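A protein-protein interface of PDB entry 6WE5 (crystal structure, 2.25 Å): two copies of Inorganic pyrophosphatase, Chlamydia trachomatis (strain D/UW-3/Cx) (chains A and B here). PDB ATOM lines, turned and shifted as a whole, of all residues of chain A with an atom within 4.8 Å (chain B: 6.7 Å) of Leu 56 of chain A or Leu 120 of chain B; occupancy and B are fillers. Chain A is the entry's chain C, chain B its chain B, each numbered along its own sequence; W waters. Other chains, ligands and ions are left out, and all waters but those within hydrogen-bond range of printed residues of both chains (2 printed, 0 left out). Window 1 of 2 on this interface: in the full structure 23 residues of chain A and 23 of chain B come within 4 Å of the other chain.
The side-chain sulfur (SG) of Cys 34 of chain B is in hydrogen-bond range of the side-chain amino group (NZ) of Lys 57 of chain A, 3.4 Å away.
The backbone NH of Leu 120 of chain B sits at hydrogen-bond distance from the backbone carbonyl oxygen of Leu 56 of chain A (2.9 Å).
The backbone carbonyl oxygen (O) of Leu 120 of chain B lies within hydrogen-bond range of the backbone NH (N) of Val 58 of chain A.
The side-chain amide oxygen of Gln 122 of chain B lies within hydrogen-bond range of the side-chain amino group of Lys 57 of chain A (2.7 Å).
Asn 118 of chain B touches its own counterpart, Asn 118 of chain A.
Positions printed for both chains: 36 and 118.
Of the 18 pairs that touch across the chains among the printed residues, 1 has its exchanged pair printed and touching as well.
Water W1 lies within hydrogen-bond range of O of Glu 38 of chain A (2.9 Å), NE2 of Gln 116 of chain B (3.0 Å) and N of Gly 117 of chain A (3.2 Å).
Water W2 bridges ND2 of Asn 118 of chain B and ND2 of Asn 118 of chain A.
Asp 50 of chain A touches none of the printed residues of chain B.
Leu 56 of chain A touches just these residues of chain B: Ile 119 and Leu 120.
Of the printed residues of chain A, Ile 16 of chain B touches Thr 53 (3.4 Å), Gly 54 (3.6 Å) and Ile 55 (3.8 Å).
Printed residues of chain A within 4 Å of Pro 23 of chain B: Thr 53.
Of the printed residues of chain A, Cys 34 of chain B touches Lys 57 (3.4 Å).
Cys 35 of chain B touches none of the printed residues of chain A.
Of the printed residues of chain A, Gln 116 of chain B touches Phe 47 and Gly 117.
Leu 120 of chain B touches just these residues of chain A: Thr 53, Ile 55, Leu 56, Lys 57 and Val 58.
The nearest residue of chain A that does not touch Leu 120 of chain B is Asp 50 of chain A (4.3 Å).
The nearest printed residue of chain A that does not touch Ile 16 of chain B is Asn 118 of chain A (5.4 Å).
Among the printed residues, merely in contact across the chains: Phe 47 of chain A with Gln 116 of chain B (3.9 Å), Phe 47 of chain A with Ile 119 of chain B (3.8 Å), Thr 53 of chain A with Ile 16 of chain B (3.4 Å), Thr 53 of chain A with Pro 23 of chain B (3.8 Å), Thr 53 of chain A with Leu 120 of chain B (3.6 Å), Gly 54 of chain A with Ile 16 of chain B (3.6 Å), Ile 55 of chain A with Ile 16 of chain B (3.8 Å), Ile 55 of chain A with Pro 19 of chain B (3.9 Å), Ile 55 of chain A with Leu 120 of chain B (3.8 Å), Leu 56 of chain A with Ile 119 of chain B (3.4 Å), Lys 57 of chain A with Leu 120 of chain B (3.3 Å), Val 58 of chain A with Leu 121 of chain B (3.8 Å), Gly 117 of chain A with Gln 116 of chain B (3.8 Å) and Asn 118 of chain A with Asn 118 of chain B (3.7 Å).
Of the 14 printed residues of chain A, 9 touch a printed residue of chain B.
Printed residues of chain A that touch a printed residue of chain B: Phe 47, Thr 53, Gly 54, Ile 55, Leu 56, Lys 57, Val 58, Gly 117 and Asn 118.
Hydrophobic or aromatic side chains of chain A within 4 Å of the printed part of chain B: Phe 47, Ile 55 and Val 58.
Of the 14 printed residues of chain B, 10 touch a printed residue of chain A.
Printed residues of chain B that touch a printed residue of chain A: Ile 16, Pro 19, Pro 23, Cys 34, Gln 116, Asn 118, Ile 119, Leu 120, Leu 121 and Gln 122.
Hydrophobic or aromatic side chains of chain B that line the printed part of chain A: Ile 16, Pro 19, Pro 23, Ile 119, Leu 120 and Leu 121.
Among the printed residues, 18 pairs touch across the chains.
Among the printed residues, no Asp or Glu carboxylate lies within 4 Å of a Lys or Arg side-chain nitrogen of the other chain.
O of Leu 121 of chain B is in hydrogen-bond range of N of Cys 35 of chain B (2.8 Å).
OD1 of Asn 118 of chain B lies within hydrogen-bond range of OH of Tyr 36 of chain B (2.6 Å).
OD1 of Asn 118 of chain A is in hydrogen-bond range of OH of Tyr 36 of chain A, 2.6 Å away.
O of Lys 57 of chain A is in hydrogen-bond range of N of Glu 48 of chain A (2.8 Å).
N of Asp 50 of chain A lies within hydrogen-bond range of O of Ile 55 of chain A (2.9 Å).
N of Ile 55 of chain A sits close to OG1 of Thr 53 of chain A (3.2 Å).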
ATOM      1  N   TYR A  36      -1.696   2.522   7.948  1.00  0.00           N
ATOM      2  CA  TYR A  36      -1.145   2.391   6.604  1.00  0.00           C
ATOM      3  C   TYR A  36      -2.245   1.966   5.632  1.00  0.00           C
ATOM      4  O   TYR A  36      -2.812   0.877   5.769  1.00  0.00           O
ATOM      5  CB  TYR A  36       0.006   1.387   6.575  1.00  0.00           C
ATOM      6  CG  TYR A  36       0.583   1.208   5.188  1.00  0.00           C
ATOM      7  CD1 TYR A  36       1.371   2.194   4.615  1.00  0.00           C
ATOM      8  CD2 TYR A  36       0.338   0.055   4.456  1.00  0.00           C
ATOM      9  CE1 TYR A  36       1.901   2.038   3.340  1.00  0.00           C
ATOM     10  CE2 TYR A  36       0.861  -0.117   3.185  1.00  0.00           C
ATOM     11  CZ  TYR A  36       1.636   0.878   2.632  1.00  0.00           C
ATOM     12  OH  TYR A  36       2.161   0.699   1.380  1.00  0.00           O
ATOM     13  N   GLU A  38      -3.842   0.659   2.241  1.00  0.00           N
ATOM     14  CA  GLU A  38      -3.505  -0.185   1.105  1.00  0.00           C
ATOM     15  C   GLU A  38      -4.450  -0.029  -0.071  1.00  0.00           C
ATOM     16  O   GLU A  38      -4.013  -0.189  -1.205  1.00  0.00           O
ATOM     17  CB  GLU A  38      -3.490  -1.663   1.503  1.00  0.00           C
ATOM     18  CG  GLU A  38      -2.625  -2.011   2.712  1.00  0.00           C
ATOM     19  CD  GLU A  38      -2.949  -3.397   3.223  1.00  0.00           C
ATOM     20  OE1 GLU A  38      -4.119  -3.609   3.598  1.00  0.00           O
ATOM     21  OE2 GLU A  38      -2.068  -4.275   3.229  1.00  0.00           O
ATOM     22  N   PHE A  47      -5.020  -4.273  -3.270  1.00  0.00           N
ATOM     23  CA  PHE A  47      -3.619  -4.168  -2.889  1.00  0.00           C
ATOM     24  C   PHE A  47      -3.414  -4.715  -1.481  1.00  0.00           C
ATOM     25  O   PHE A  47      -4.324  -4.705  -0.653  1.00  0.00           O
ATOM     26  CB  PHE A  47      -3.142  -2.715  -2.936  1.00  0.00           C
ATOM     27  CG  PHE A  47      -3.090  -2.119  -4.324  1.00  0.00           C
ATOM     28  CD1 PHE A  47      -2.032  -2.382  -5.166  1.00  0.00           C
ATOM     29  CD2 PHE A  47      -4.102  -1.275  -4.771  1.00  0.00           C
ATOM     30  CE1 PHE A  47      -1.974  -1.816  -6.439  1.00  0.00           C
ATOM     31  CE2 PHE A  47      -4.048  -0.707  -6.042  1.00  0.00           C
ATOM     32  CZ  PHE A  47      -2.984  -0.982  -6.874  1.00  0.00           C
ATOM     33  N   GLU A  48      -2.195  -5.172  -1.212  1.00  0.00           N
ATOM     34  CA  GLU A  48      -1.813  -5.618   0.120  1.00  0.00           C
ATOM     35  C   GLU A  48      -0.324  -5.359   0.289  1.00  0.00           C
ATOM     36  O   GLU A  48       0.465  -5.632  -0.617  1.00  0.00           O
ATOM     37  CB  GLU A  48      -2.127  -7.103   0.343  1.00  0.00           C
ATOM     38  N   LEU A  49       0.052  -4.838   1.452  1.00  0.00           N
ATOM     39  CA  LEU A  49       1.462  -4.611   1.743  1.00  0.00           C
ATOM     40  C   LEU A  49       2.222  -5.924   1.681  1.00  0.00           C
ATOM     41  O   LEU A  49       1.843  -6.899   2.336  1.00  0.00           O
ATOM     42  CB  LEU A  49       1.620  -3.973   3.123  1.00  0.00           C
ATOM     43  CG  LEU A  49       3.065  -3.622   3.472  1.00  0.00           C
ATOM     44  CD1 LEU A  49       3.572  -2.474   2.610  1.00  0.00           C
ATOM     45  CD2 LEU A  49       3.198  -3.285   4.946  1.00  0.00           C
ATOM     46  N   ASP A  50       3.273  -5.965   0.864  1.00  0.00           N
ATOM     47  CA  ASP A  50       4.097  -7.165   0.767  1.00  0.00           C
ATOM     48  C   ASP A  50       4.948  -7.291   2.030  1.00  0.00           C
ATOM     49  O   ASP A  50       5.824  -6.459   2.290  1.00  0.00           O
ATOM     50  CB  ASP A  50       4.965  -7.130  -0.485  1.00  0.00           C
ATOM     51  CG  ASP A  50       5.765  -8.409  -0.673  1.00  0.00           C
ATOM     52  OD1 ASP A  50       5.146  -9.489  -0.820  1.00  0.00           O
ATOM     53  OD2 ASP A  50       7.013  -8.341  -0.641  1.00  0.00           O
ATOM     54  N   THR A  53       8.929  -7.379   1.488  1.00  0.00           N
ATOM     55  CA  THR A  53       9.644  -6.210   0.999  1.00  0.00           C
ATOM     56  C   THR A  53       9.123  -4.906   1.575  1.00  0.00           C
ATOM     57  O   THR A  53       9.862  -3.917   1.589  1.00  0.00           O
ATOM     58  CB  THR A  53       9.585  -6.157  -0.532  1.00  0.00           C
ATOM     59  OG1 THR A  53       8.243  -5.887  -0.956  1.00  0.00           O
ATOM     60  CG2 THR A  53      10.039  -7.492  -1.121  1.00  0.00           C
ATOM     61  N   GLY A  54       7.893  -4.885   2.086  1.00  0.00           N
ATOM     62  CA  GLY A  54       7.344  -3.619   2.510  1.00  0.00           C
ATOM     63  C   GLY A  54       6.908  -2.714   1.377  1.00  0.00           C
ATOM     64  O   GLY A  54       6.693  -1.522   1.612  1.00  0.00           O
ATOM     65  N   ILE A  55       6.815  -3.231   0.147  1.00  0.00           N
ATOM     66  CA  ILE A  55       6.283  -2.498  -1.001  1.00  0.00           C
ATOM     67  C   ILE A  55       4.819  -2.883  -1.190  1.00  0.00           C
ATOM     68  O   ILE A  55       4.450  -4.052  -1.029  1.00  0.00           O
ATOM     69  CB  ILE A  55       7.095  -2.802  -2.277  1.00  0.00           C
ATOM     70  CG1 ILE A  55       8.580  -2.533  -2.060  1.00  0.00           C
ATOM     71  CG2 ILE A  55       6.603  -1.955  -3.453  1.00  0.00           C
ATOM     72  CD1 ILE A  55       9.423  -2.883  -3.253  1.00  0.00           C
ATOM     73  N   LEU A  56       3.980  -1.912  -1.542  1.00  0.00           N
ATOM     74  CA  LEU A  56       2.592  -2.226  -1.851  1.00  0.00           C
ATOM     75  C   LEU A  56       2.543  -3.114  -3.089  1.00  0.00           C
ATOM     76  O   LEU A  56       3.286  -2.904  -4.050  1.00  0.00           O
ATOM     77  CB  LEU A  56       1.774  -0.952  -2.071  1.00  0.00           C
ATOM     78  CG  LEU A  56       0.253  -1.128  -1.914  1.00  0.00           C
ATOM     79  CD1 LEU A  56      -0.111  -1.587  -0.490  1.00  0.00           C
ATOM     80  CD2 LEU A  56      -0.569   0.121  -2.308  1.00  0.00           C
ATOM     81  N   LYS A  57       1.699  -4.145  -3.039  1.00  0.00           N
ATOM     82  CA  LYS A  57       1.651  -5.179  -4.064  1.00  0.00           C
ATOM     83  C   LYS A  57       0.212  -5.492  -4.446  1.00  0.00           C
ATOM     84  O   LYS A  57      -0.678  -5.507  -3.592  1.00  0.00           O
ATOM     85  CB  LYS A  57       2.335  -6.463  -3.573  1.00  0.00           C
ATOM     86  CG  LYS A  57       2.392  -7.594  -4.588  1.00  0.00           C
ATOM     87  CD  LYS A  57       3.522  -8.568  -4.247  1.00  0.00           C
ATOM     88  CE  LYS A  57       3.669  -9.663  -5.296  1.00  0.00           C
ATOM     89  NZ  LYS A  57       4.944 -10.423  -5.135  1.00  0.00           N
ATOM     90  N   VAL A  58      -0.009  -5.764  -5.729  1.00  0.00           N
ATOM     91  CA  VAL A  58      -1.314  -6.236  -6.168  1.00  0.00           C
ATOM     92  C   VAL A  58      -1.528  -7.648  -5.641  1.00  0.00           C
ATOM     93  O   VAL A  58      -0.767  -8.569  -5.963  1.00  0.00           O
ATOM     94  CB  VAL A  58      -1.434  -6.187  -7.698  1.00  0.00           C
ATOM     95  CG1 VAL A  58      -2.724  -6.849  -8.138  1.00  0.00           C
ATOM     96  CG2 VAL A  58      -1.390  -4.754  -8.188  1.00  0.00           C
ATOM     97  N   GLY A 117      -3.147   4.586  -2.440  1.00  0.00           N
ATOM     98  CA  GLY A 117      -2.722   4.027  -1.170  1.00  0.00           C
ATOM     99  C   GLY A 117      -1.238   4.254  -0.953  1.00  0.00           C
ATOM    100  O   GLY A 117      -0.649   5.204  -1.480  1.00  0.00           O
ATOM    101  N   ASN A 118      -0.613   3.359  -0.184  1.00  0.00           N
ATOM    102  CA  ASN A 118       0.803   3.494   0.197  1.00  0.00           C
ATOM    103  C   ASN A 118       1.061   4.819   0.918  1.00  0.00           C
ATOM    104  O   ASN A 118       1.987   5.561   0.591  1.00  0.00           O
ATOM    105  CB  ASN A 118       1.732   3.350  -1.016  1.00  0.00           C
ATOM    106  CG  ASN A 118       3.189   3.159  -0.619  1.00  0.00           C
ATOM    107  OD1 ASN A 118       3.486   2.729   0.496  1.00  0.00           O
ATOM    108  ND2 ASN A 118       4.107   3.509  -1.526  1.00  0.00           N
ATOM    109  N   ILE B  16      11.860  -0.664   3.934  1.00  0.00           N
ATOM    110  CA  ILE B  16      11.304  -1.055   2.647  1.00  0.00           C
ATOM    111  C   ILE B  16      12.440  -1.462   1.723  1.00  0.00           C
ATOM    112  O   ILE B  16      13.455  -0.763   1.626  1.00  0.00           O
ATOM    113  CB  ILE B  16      10.498   0.095   2.025  1.00  0.00           C
ATOM    114  CG1 ILE B  16       9.386   0.565   2.960  1.00  0.00           C
ATOM    115  CG2 ILE B  16       9.939  -0.330   0.676  1.00  0.00           C
ATOM    116  CD1 ILE B  16       8.482   1.618   2.304  1.00  0.00           C
ATOM    117  N   PRO B  19      13.243  -1.776  -4.780  1.00  0.00           N
ATOM    118  CA  PRO B  19      12.441  -2.598  -5.703  1.00  0.00           C
ATOM    119  C   PRO B  19      13.269  -3.403  -6.695  1.00  0.00           C
ATOM    120  O   PRO B  19      12.842  -4.486  -7.112  1.00  0.00           O
ATOM    121  CB  PRO B  19      11.563  -1.560  -6.422  1.00  0.00           C
ATOM    122  CG  PRO B  19      11.472  -0.419  -5.461  1.00  0.00           C
ATOM    123  CD  PRO B  19      12.832  -0.362  -4.802  1.00  0.00           C
ATOM    124  N   PRO B  23      13.033  -7.601  -3.884  1.00  0.00           N
ATOM    125  CA  PRO B  23      12.063  -8.689  -4.074  1.00  0.00           C
ATOM    126  C   PRO B  23      12.665  -9.892  -4.785  1.00  0.00           C
ATOM    127  O   PRO B  23      13.658  -9.787  -5.506  1.00  0.00           O
ATOM    128  CB  PRO B  23      10.951  -8.046  -4.910  1.00  0.00           C
ATOM    129  CG  PRO B  23      11.440  -6.703  -5.297  1.00  0.00           C
ATOM    130  CD  PRO B  23      12.522  -6.309  -4.368  1.00  0.00           C
ATOM    131  N   CYS B  34       7.541 -11.607 -10.118  1.00  0.00           N
ATOM    132  CA  CYS B  34       7.283 -10.382  -9.378  1.00  0.00           C
ATOM    133  C   CYS B  34       7.777  -9.199 -10.201  1.00  0.00           C
ATOM    134  O   CYS B  34       8.929  -9.185 -10.638  1.00  0.00           O
ATOM    135  CB  CYS B  34       7.989 -10.430  -8.022  1.00  0.00           C
ATOM    136  SG  CYS B  34       7.590  -9.086  -6.892  1.00  0.00           S
ATOM    137  N   CYS B  35       6.906  -8.216 -10.430  1.00  0.00           N
ATOM    138  CA  CYS B  35       7.217  -7.077 -11.284  1.00  0.00           C
ATOM    139  C   CYS B  35       7.042  -5.783 -10.507  1.00  0.00           C
ATOM    140  O   CYS B  35       6.091  -5.644  -9.734  1.00  0.00           O
ATOM    141  CB  CYS B  35       6.306  -7.042 -12.513  1.00  0.00           C
ATOM    142  SG  CYS B  35       6.102  -8.615 -13.345  1.00  0.00           S
ATOM    143  N   TYR B  36       7.939  -4.828 -10.740  1.00  0.00           N
ATOM    144  CA  TYR B  36       7.822  -3.486 -10.181  1.00  0.00           C
ATOM    145  C   TYR B  36       7.378  -2.516 -11.276  1.00  0.00           C
ATOM    146  O   TYR B  36       8.090  -2.321 -12.265  1.00  0.00           O
ATOM    147  CB  TYR B  36       9.144  -3.038  -9.562  1.00  0.00           C
ATOM    148  CG  TYR B  36       9.102  -1.629  -9.036  1.00  0.00           C
ATOM    149  CD1 TYR B  36       8.406  -1.315  -7.861  1.00  0.00           C
ATOM    150  CD2 TYR B  36       9.747  -0.606  -9.714  1.00  0.00           C
ATOM    151  CE1 TYR B  36       8.355  -0.008  -7.392  1.00  0.00           C
ATOM    152  CE2 TYR B  36       9.700   0.700  -9.251  1.00  0.00           C
ATOM    153  CZ  TYR B  36       9.009   0.993  -8.095  1.00  0.00           C
ATOM    154  OH  TYR B  36       8.986   2.292  -7.654  1.00  0.00           O
ATOM    155  N   ILE B  37       6.224  -1.893 -11.089  1.00  0.00           N
ATOM    156  CA  ILE B  37       5.609  -1.074 -12.132  1.00  0.00           C
ATOM    157  C   ILE B  37       6.031   0.377 -11.969  1.00  0.00           C
ATOM    158  O   ILE B  37       5.843   0.977 -10.905  1.00  0.00           O
ATOM    159  CB  ILE B  37       4.082  -1.209 -12.105  1.00  0.00           C
ATOM    160  CG1 ILE B  37       3.684  -2.685 -12.244  1.00  0.00           C
ATOM    161  CG2 ILE B  37       3.464  -0.381 -13.213  1.00  0.00           C
ATOM    162  CD1 ILE B  37       4.299  -3.384 -13.448  1.00  0.00           C
ATOM    163  N   PRO B  76      12.699  -7.390 -10.963  1.00  0.00           N
ATOM    164  CA  PRO B  76      13.724  -7.393  -9.916  1.00  0.00           C
ATOM    165  C   PRO B  76      14.812  -8.419 -10.181  1.00  0.00           C
ATOM    166  O   PRO B  76      14.583  -9.454 -10.811  1.00  0.00           O
ATOM    167  CB  PRO B  76      12.927  -7.734  -8.650  1.00  0.00           C
ATOM    168  CG  PRO B  76      11.579  -7.153  -8.924  1.00  0.00           C
ATOM    169  CD  PRO B  76      11.339  -7.397 -10.398  1.00  0.00           C
ATOM    170  N   GLN B 116      -1.722   4.227 -10.358  1.00  0.00           N
ATOM    171  CA  GLN B 116      -0.473   4.556  -9.687  1.00  0.00           C
ATOM    172  C   GLN B 116       0.584   3.502  -9.983  1.00  0.00           C
ATOM    173  O   GLN B 116       0.303   2.300  -9.961  1.00  0.00           O
ATOM    174  CB  GLN B 116      -0.685   4.648  -8.170  1.00  0.00           C
ATOM    175  CG  GLN B 116      -1.345   3.403  -7.561  1.00  0.00           C
ATOM    176  CD  GLN B 116      -1.126   3.278  -6.055  1.00  0.00           C
ATOM    177  OE1 GLN B 116      -0.225   3.903  -5.487  1.00  0.00           O
ATOM    178  NE2 GLN B 116      -1.954   2.463  -5.403  1.00  0.00           N
ATOM    179  N   ASN B 118       4.817   2.582  -8.841  1.00  0.00           N
ATOM    180  CA  ASN B 118       5.492   2.293  -7.572  1.00  0.00           C
ATOM    181  C   ASN B 118       4.795   1.161  -6.809  1.00  0.00           C
ATOM    182  O   ASN B 118       4.515   1.272  -5.612  1.00  0.00           O
ATOM    183  CB  ASN B 118       5.609   3.540  -6.689  1.00  0.00           C
ATOM    184  CG  ASN B 118       6.559   3.330  -5.517  1.00  0.00           C
ATOM    185  OD1 ASN B 118       7.428   2.460  -5.564  1.00  0.00           O
ATOM    186  ND2 ASN B 118       6.361   4.085  -4.441  1.00  0.00           N
ATOM    187  N   ILE B 119       4.504   0.063  -7.516  1.00  0.00           N
ATOM    188  CA  ILE B 119       3.851  -1.102  -6.924  1.00  0.00           C
ATOM    189  C   ILE B 119       4.486  -2.365  -7.481  1.00  0.00           C
ATOM    190  O   ILE B 119       5.105  -2.362  -8.548  1.00  0.00           O
ATOM    191  CB  ILE B 119       2.332  -1.158  -7.179  1.00  0.00           C
ATOM    192  CG1 ILE B 119       2.075  -1.103  -8.693  1.00  0.00           C
ATOM    193  CG2 ILE B 119       1.634  -0.036  -6.414  1.00  0.00           C
ATOM    194  CD1 ILE B 119       0.694  -1.455  -9.136  1.00  0.00           C
ATOM    195  N   LEU B 120       4.298  -3.456  -6.745  1.00  0.00           N
ATOM    196  CA  LEU B 120       4.644  -4.801  -7.172  1.00  0.00           C
ATOM    197  C   LEU B 120       3.385  -5.517  -7.648  1.00  0.00           C
ATOM    198  O   LEU B 120       2.270  -5.172  -7.263  1.00  0.00           O
ATOM    199  CB  LEU B 120       5.282  -5.590  -6.016  1.00  0.00           C
ATOM    200  CG  LEU B 120       6.635  -5.181  -5.439  1.00  0.00           C
ATOM    201  CD1 LEU B 120       7.015  -6.113  -4.284  1.00  0.00           C
ATOM    202  CD2 LEU B 120       7.730  -5.191  -6.513  1.00  0.00           C
ATOM    203  N   LEU B 121       3.577  -6.518  -8.502  1.00  0.00           N
ATOM    204  CA  LEU B 121       2.484  -7.402  -8.894  1.00  0.00           C
ATOM    205  C   LEU B 121       3.079  -8.688  -9.445  1.00  0.00           C
ATOM    206  O   LEU B 121       4.247  -8.731  -9.837  1.00  0.00           O
ATOM    207  CB  LEU B 121       1.539  -6.744  -9.920  1.00  0.00           C
ATOM    208  CG  LEU B 121       2.087  -6.170 -11.233  1.00  0.00           C
ATOM    209  CD1 LEU B 121       2.464  -7.262 -12.214  1.00  0.00           C
ATOM    210  CD2 LEU B 121       1.038  -5.268 -11.862  1.00  0.00           C
ATOM    211  N   GLN B 122       2.254  -9.727  -9.487  1.00  0.00           N
ATOM    212  CA  GLN B 122       2.627 -11.012 -10.057  1.00  0.00           C
ATOM    213  C   GLN B 122       2.076 -11.117 -11.472  1.00  0.00           C
ATOM    214  O   GLN B 122       0.896 -10.842 -11.707  1.00  0.00           O
ATOM    215  CB  GLN B 122       2.108 -12.165  -9.199  1.00  0.00           C
ATOM    216  CG  GLN B 122       2.785 -12.292  -7.835  1.00  0.00           C
ATOM    217  CD  GLN B 122       4.251 -12.681  -7.923  1.00  0.00           C
ATOM    218  OE1 GLN B 122       5.115 -12.025  -7.335  1.00  0.00           O
ATOM    219  NE2 GLN B 122       4.540 -13.750  -8.656  1.00  0.00           N
HETATM  220  O   HOH W   1      -4.118   1.729  -3.391  1.00  0.00           O
HETATM  221  O   HOH W   2       3.688   5.335  -3.886  1.00  0.00           O
